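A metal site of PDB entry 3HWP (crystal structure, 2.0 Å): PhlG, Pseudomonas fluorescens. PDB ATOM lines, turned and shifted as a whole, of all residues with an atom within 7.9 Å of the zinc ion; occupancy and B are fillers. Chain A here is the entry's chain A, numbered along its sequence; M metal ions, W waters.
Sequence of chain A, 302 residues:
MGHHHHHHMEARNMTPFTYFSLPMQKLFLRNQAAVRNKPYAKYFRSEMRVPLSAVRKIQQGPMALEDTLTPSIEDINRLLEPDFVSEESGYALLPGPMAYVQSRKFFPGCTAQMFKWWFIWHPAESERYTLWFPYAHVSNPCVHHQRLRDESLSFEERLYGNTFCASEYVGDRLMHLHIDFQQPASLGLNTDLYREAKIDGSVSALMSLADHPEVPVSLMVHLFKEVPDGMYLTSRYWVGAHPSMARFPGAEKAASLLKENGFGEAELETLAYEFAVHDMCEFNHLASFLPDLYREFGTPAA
The backbone carbonyl oxygen (O) of Glu 282 sits close to the indole nitrogen (NE1) of Trp 132. ND1 of His 278 sits at hydrogen-bond distance from O of Tyr 169 (3.1 Å). A ring nitrogen (ND1) of His 137 sits at hydrogen-bond distance from the backbone carbonyl oxygen (O) of Tyr 129 (3.0 Å). The side-chain carboxylate (OE1) of Glu 168 sits close to the side-chain hydroxyl (OH) of Tyr 129, 3.3 Å away.
Within 4 Å of the zinc ion: His 137, Glu 168, His 278 and Glu 282.
The zinc ion is bound by a ring nitrogen (NE2) of His 137 (2.1 Å), the side-chain carboxylate (OE1) of Glu 282 (2.1 Å), a ring nitrogen (NE2) of His 278 (2.2 Å), the side-chain carboxylate (OE1) of Glu 168 (2.2 Å) and water W1 (2.3 Å). The zinc ion has five donor atoms within binding distance.
Water W1 bridges the side-chain carboxylate (OE2) of Glu 168 and the side-chain carboxylate (OE2) of Glu 282.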
ATOM      1  N   TYR A 129       7.151  26.136  21.668  1.00  0.00           N
ATOM      2  CA  TYR A 129       5.779  26.470  21.322  1.00  0.00           C
ATOM      3  C   TYR A 129       5.704  26.978  19.870  1.00  0.00           C
ATOM      4  O   TYR A 129       4.754  26.692  19.135  1.00  0.00           O
ATOM      5  CB  TYR A 129       5.239  27.503  22.307  1.00  0.00           C
ATOM      6  CG  TYR A 129       3.776  27.858  22.209  1.00  0.00           C
ATOM      7  CD1 TYR A 129       2.793  26.876  22.152  1.00  0.00           C
ATOM      8  CD2 TYR A 129       3.376  29.191  22.203  1.00  0.00           C
ATOM      9  CE1 TYR A 129       1.453  27.208  22.080  1.00  0.00           C
ATOM     10  CE2 TYR A 129       2.033  29.544  22.125  1.00  0.00           C
ATOM     11  CZ  TYR A 129       1.071  28.548  22.063  1.00  0.00           C
ATOM     12  OH  TYR A 129      -0.264  28.901  21.977  1.00  0.00           O
ATOM     13  N   TRP A 132       5.352  24.440  16.774  1.00  0.00           N
ATOM     14  CA  TRP A 132       3.985  23.961  16.572  1.00  0.00           C
ATOM     15  C   TRP A 132       3.249  24.815  15.531  1.00  0.00           C
ATOM     16  O   TRP A 132       2.507  24.296  14.672  1.00  0.00           O
ATOM     17  CB  TRP A 132       3.283  24.054  17.928  1.00  0.00           C
ATOM     18  CG  TRP A 132       1.998  23.305  18.085  1.00  0.00           C
ATOM     19  CD1 TRP A 132       1.298  22.643  17.111  1.00  0.00           C
ATOM     20  CD2 TRP A 132       1.249  23.181  19.291  1.00  0.00           C
ATOM     21  NE1 TRP A 132       0.152  22.100  17.654  1.00  0.00           N
ATOM     22  CE2 TRP A 132       0.099  22.416  18.985  1.00  0.00           C
ATOM     23  CE3 TRP A 132       1.428  23.650  20.596  1.00  0.00           C
ATOM     24  CZ2 TRP A 132      -0.851  22.098  19.950  1.00  0.00           C
ATOM     25  CZ3 TRP A 132       0.485  23.321  21.553  1.00  0.00           C
ATOM     26  CH2 TRP A 132      -0.643  22.553  21.228  1.00  0.00           C
ATOM     27  N   PHE A 133       3.454  26.119  15.578  1.00  0.00           N
ATOM     28  CA  PHE A 133       2.784  27.036  14.653  1.00  0.00           C
ATOM     29  C   PHE A 133       3.644  28.285  14.523  1.00  0.00           C
ATOM     30  O   PHE A 133       3.391  29.297  15.181  1.00  0.00           O
ATOM     31  CB  PHE A 133       1.381  27.373  15.179  1.00  0.00           C
ATOM     32  CG  PHE A 133       0.424  27.871  14.114  1.00  0.00           C
ATOM     33  CD1 PHE A 133      -0.947  27.875  14.352  1.00  0.00           C
ATOM     34  CD2 PHE A 133       0.881  28.363  12.894  1.00  0.00           C
ATOM     35  CE1 PHE A 133      -1.840  28.354  13.414  1.00  0.00           C
ATOM     36  CE2 PHE A 133      -0.013  28.823  11.926  1.00  0.00           C
ATOM     37  CZ  PHE A 133      -1.374  28.814  12.179  1.00  0.00           C
ATOM     38  N   ALA A 136       1.928  31.777  14.277  1.00  0.00           N
ATOM     39  CA  ALA A 136       0.853  32.207  15.182  1.00  0.00           C
ATOM     40  C   ALA A 136       1.211  32.197  16.662  1.00  0.00           C
ATOM     41  O   ALA A 136       0.597  32.919  17.448  1.00  0.00           O
ATOM     42  CB  ALA A 136      -0.415  31.378  14.932  1.00  0.00           C
ATOM     43  N   HIS A 137       2.179  31.372  17.052  1.00  0.00           N
ATOM     44  CA  HIS A 137       2.453  31.196  18.474  1.00  0.00           C
ATOM     45  C   HIS A 137       3.496  32.138  19.033  1.00  0.00           C
ATOM     46  O   HIS A 137       4.545  32.355  18.437  1.00  0.00           O
ATOM     47  CB  HIS A 137       2.847  29.746  18.773  1.00  0.00           C
ATOM     48  CG  HIS A 137       1.706  28.783  18.680  1.00  0.00           C
ATOM     49  ND1 HIS A 137       1.878  27.421  18.668  1.00  0.00           N
ATOM     50  CD2 HIS A 137       0.374  28.993  18.589  1.00  0.00           C
ATOM     51  CE1 HIS A 137       0.703  26.830  18.573  1.00  0.00           C
ATOM     52  NE2 HIS A 137      -0.233  27.762  18.517  1.00  0.00           N
ATOM     53  N   VAL A 138       3.204  32.688  20.215  1.00  0.00           N
ATOM     54  CA  VAL A 138       4.180  33.522  20.897  1.00  0.00           C
ATOM     55  C   VAL A 138       4.754  32.778  22.105  1.00  0.00           C
ATOM     56  O   VAL A 138       5.939  32.436  22.118  1.00  0.00           O
ATOM     57  CB  VAL A 138       3.583  34.872  21.342  1.00  0.00           C
ATOM     58  CG1 VAL A 138       4.659  35.731  22.000  1.00  0.00           C
ATOM     59  CG2 VAL A 138       2.965  35.582  20.150  1.00  0.00           C
ATOM     60  N   ALA A 166      -1.569  31.066  27.158  1.00  0.00           N
ATOM     61  CA  ALA A 166      -1.194  31.054  25.759  1.00  0.00           C
ATOM     62  C   ALA A 166      -1.351  32.442  25.126  1.00  0.00           C
ATOM     63  O   ALA A 166      -2.392  33.087  25.240  1.00  0.00           O
ATOM     64  CB  ALA A 166      -2.017  30.025  24.991  1.00  0.00           C
ATOM     65  N   SER A 167      -0.290  32.904  24.478  1.00  0.00           N
ATOM     66  CA  SER A 167      -0.354  34.114  23.670  1.00  0.00           C
ATOM     67  C   SER A 167      -0.158  33.667  22.248  1.00  0.00           C
ATOM     68  O   SER A 167       0.866  33.058  21.921  1.00  0.00           O
ATOM     69  CB  SER A 167       0.739  35.097  24.079  1.00  0.00           C
ATOM     70  OG  SER A 167       0.560  35.516  25.416  1.00  0.00           O
ATOM     71  N   GLU A 168      -1.154  33.935  21.390  1.00  0.00           N
ATOM     72  CA  GLU A 168      -1.109  33.472  20.009  1.00  0.00           C
ATOM     73  C   GLU A 168      -2.108  34.239  19.150  1.00  0.00           C
ATOM     74  O   GLU A 168      -3.143  34.718  19.641  1.00  0.00           O
ATOM     75  CB  GLU A 168      -1.404  31.972  19.929  1.00  0.00           C
ATOM     76  CG  GLU A 168      -2.817  31.606  20.360  1.00  0.00           C
ATOM     77  CD  GLU A 168      -3.060  30.099  20.407  1.00  0.00           C
ATOM     78  OE1 GLU A 168      -2.513  29.373  19.556  1.00  0.00           O
ATOM     79  OE2 GLU A 168      -3.798  29.636  21.301  1.00  0.00           O
ATOM     80  N   TYR A 169      -1.806  34.365  17.863  1.00  0.00           N
ATOM     81  CA  TYR A 169      -2.739  34.933  16.910  1.00  0.00           C
ATOM     82  C   TYR A 169      -3.756  33.887  16.492  1.00  0.00           C
ATOM     83  O   TYR A 169      -3.405  32.720  16.257  1.00  0.00           O
ATOM     84  CB  TYR A 169      -2.000  35.417  15.668  1.00  0.00           C
ATOM     85  CG  TYR A 169      -1.345  36.757  15.828  1.00  0.00           C
ATOM     86  CD1 TYR A 169      -2.029  37.923  15.537  1.00  0.00           C
ATOM     87  CD2 TYR A 169      -0.035  36.845  16.270  1.00  0.00           C
ATOM     88  CE1 TYR A 169      -1.437  39.152  15.685  1.00  0.00           C
ATOM     89  CE2 TYR A 169       0.577  38.070  16.427  1.00  0.00           C
ATOM     90  CZ  TYR A 169      -0.132  39.220  16.141  1.00  0.00           C
ATOM     91  OH  TYR A 169       0.480  40.436  16.283  1.00  0.00           O
ATOM     92  N   VAL A 170      -5.004  34.304  16.440  1.00  0.00           N
ATOM     93  CA  VAL A 170      -6.068  33.576  15.760  1.00  0.00           C
ATOM     94  C   VAL A 170      -6.526  34.479  14.621  1.00  0.00           C
ATOM     95  O   VAL A 170      -7.224  35.474  14.841  1.00  0.00           O
ATOM     96  CB  VAL A 170      -7.250  33.271  16.680  1.00  0.00           C
ATOM     97  CG1 VAL A 170      -8.332  32.522  15.919  1.00  0.00           C
ATOM     98  CG2 VAL A 170      -6.792  32.437  17.872  1.00  0.00           C
ATOM     99  N   LEU A 177      -4.928  33.734  25.977  1.00  0.00           N
ATOM    100  CA  LEU A 177      -5.899  32.786  26.492  1.00  0.00           C
ATOM    101  C   LEU A 177      -5.320  32.071  27.702  1.00  0.00           C
ATOM    102  O   LEU A 177      -4.166  31.665  27.688  1.00  0.00           O
ATOM    103  CB  LEU A 177      -6.277  31.779  25.408  1.00  0.00           C
ATOM    104  CG  LEU A 177      -6.795  32.436  24.124  1.00  0.00           C
ATOM    105  CD1 LEU A 177      -7.068  31.410  23.043  1.00  0.00           C
ATOM    106  CD2 LEU A 177      -8.048  33.239  24.429  1.00  0.00           C
ATOM    107  N   ILE A 179      -5.641  28.757  29.606  1.00  0.00           N
ATOM    108  CA  ILE A 179      -6.141  27.431  29.285  1.00  0.00           C
ATOM    109  C   ILE A 179      -5.995  26.518  30.492  1.00  0.00           C
ATOM    110  O   ILE A 179      -4.874  26.243  30.935  1.00  0.00           O
ATOM    111  CB  ILE A 179      -5.377  26.849  28.093  1.00  0.00           C
ATOM    112  CG1 ILE A 179      -5.496  27.797  26.898  1.00  0.00           C
ATOM    113  CG2 ILE A 179      -5.870  25.440  27.762  1.00  0.00           C
ATOM    114  CD1 ILE A 179      -4.741  27.342  25.660  1.00  0.00           C
ATOM    115  N   TYR A 237     -14.302  22.889  19.533  1.00  0.00           N
ATOM    116  CA  TYR A 237     -14.064  24.194  20.140  1.00  0.00           C
ATOM    117  C   TYR A 237     -15.381  24.948  20.251  1.00  0.00           C
ATOM    118  O   TYR A 237     -16.114  25.055  19.278  1.00  0.00           O
ATOM    119  CB  TYR A 237     -13.124  25.026  19.275  1.00  0.00           C
ATOM    120  CG  TYR A 237     -11.732  24.478  19.066  1.00  0.00           C
ATOM    121  CD1 TYR A 237     -11.488  23.420  18.185  1.00  0.00           C
ATOM    122  CD2 TYR A 237     -10.639  25.060  19.706  1.00  0.00           C
ATOM    123  CE1 TYR A 237     -10.210  22.953  17.967  1.00  0.00           C
ATOM    124  CE2 TYR A 237      -9.347  24.591  19.491  1.00  0.00           C
ATOM    125  CZ  TYR A 237      -9.145  23.550  18.620  1.00  0.00           C
ATOM    126  OH  TYR A 237      -7.869  23.073  18.403  1.00  0.00           O
ATOM    127  N   PHE A 275     -10.398  30.030  13.867  1.00  0.00           N
ATOM    128  CA  PHE A 275     -10.015  28.961  14.785  1.00  0.00           C
ATOM    129  C   PHE A 275      -9.886  27.642  14.010  1.00  0.00           C
ATOM    130  O   PHE A 275      -8.986  26.848  14.252  1.00  0.00           O
ATOM    131  CB  PHE A 275     -11.043  28.809  15.912  1.00  0.00           C
ATOM    132  CG  PHE A 275     -10.659  29.519  17.191  1.00  0.00           C
ATOM    133  CD1 PHE A 275     -11.344  30.652  17.610  1.00  0.00           C
ATOM    134  CD2 PHE A 275      -9.639  29.036  18.000  1.00  0.00           C
ATOM    135  CE1 PHE A 275     -10.997  31.303  18.790  1.00  0.00           C
ATOM    136  CE2 PHE A 275      -9.288  29.675  19.186  1.00  0.00           C
ATOM    137  CZ  PHE A 275      -9.968  30.819  19.579  1.00  0.00           C
ATOM    138  N   HIS A 278      -6.640  27.719  12.180  1.00  0.00           N
ATOM    139  CA  HIS A 278      -5.562  27.611  13.175  1.00  0.00           C
ATOM    140  C   HIS A 278      -5.389  26.157  13.664  1.00  0.00           C
ATOM    141  O   HIS A 278      -4.297  25.600  13.630  1.00  0.00           O
ATOM    142  CB  HIS A 278      -5.903  28.526  14.353  1.00  0.00           C
ATOM    143  CG  HIS A 278      -4.824  28.639  15.378  1.00  0.00           C
ATOM    144  ND1 HIS A 278      -4.156  29.819  15.624  1.00  0.00           N
ATOM    145  CD2 HIS A 278      -4.321  27.735  16.258  1.00  0.00           C
ATOM    146  CE1 HIS A 278      -3.277  29.636  16.595  1.00  0.00           C
ATOM    147  NE2 HIS A 278      -3.370  28.386  17.002  1.00  0.00           N
ATOM    148  N   ASP A 279      -6.484  25.580  14.133  1.00  0.00           N
ATOM    149  CA  ASP A 279      -6.504  24.184  14.555  1.00  0.00           C
ATOM    150  C   ASP A 279      -5.957  23.258  13.469  1.00  0.00           C
ATOM    151  O   ASP A 279      -5.097  22.409  13.733  1.00  0.00           O
ATOM    152  CB  ASP A 279      -7.943  23.805  14.926  1.00  0.00           C
ATOM    153  CG  ASP A 279      -8.149  22.308  15.062  1.00  0.00           C
ATOM    154  OD1 ASP A 279      -7.613  21.698  16.015  1.00  0.00           O
ATOM    155  OD2 ASP A 279      -8.895  21.747  14.237  1.00  0.00           O
ATOM    156  N   GLU A 282      -1.999  23.972  12.834  1.00  0.00           N
ATOM    157  CA  GLU A 282      -1.089  23.623  13.915  1.00  0.00           C
ATOM    158  C   GLU A 282      -1.005  22.118  14.180  1.00  0.00           C
ATOM    159  O   GLU A 282       0.085  21.579  14.360  1.00  0.00           O
ATOM    160  CB  GLU A 282      -1.388  24.391  15.212  1.00  0.00           C
ATOM    161  CG  GLU A 282      -2.583  23.913  16.016  1.00  0.00           C
ATOM    162  CD  GLU A 282      -2.840  24.800  17.237  1.00  0.00           C
ATOM    163  OE1 GLU A 282      -1.953  25.600  17.568  1.00  0.00           O
ATOM    164  OE2 GLU A 282      -3.918  24.699  17.842  1.00  0.00           O
ATOM    165  N   PHE A 283      -2.156  21.435  14.190  1.00  0.00           N
ATOM    166  CA  PHE A 283      -2.150  20.020  14.536  1.00  0.00           C
ATOM    167  C   PHE A 283      -1.625  19.119  13.420  1.00  0.00           C
ATOM    168  O   PHE A 283      -0.942  18.138  13.697  1.00  0.00           O
ATOM    169  CB  PHE A 283      -3.506  19.554  15.083  1.00  0.00           C
ATOM    170  CG  PHE A 283      -3.730  19.912  16.548  1.00  0.00           C
ATOM    171  CD1 PHE A 283      -2.963  19.330  17.554  1.00  0.00           C
ATOM    172  CD2 PHE A 283      -4.727  20.809  16.911  1.00  0.00           C
ATOM    173  CE1 PHE A 283      -3.179  19.632  18.897  1.00  0.00           C
ATOM    174  CE2 PHE A 283      -4.958  21.104  18.252  1.00  0.00           C
ATOM    175  CZ  PHE A 283      -4.167  20.528  19.240  1.00  0.00           C
HETATM  176 ZN    ZN M   1      -2.273  27.425  18.602  1.00  0.00          ZN
HETATM  177  O   HOH W   1      -2.956  26.552  20.565  1.00  0.00           O
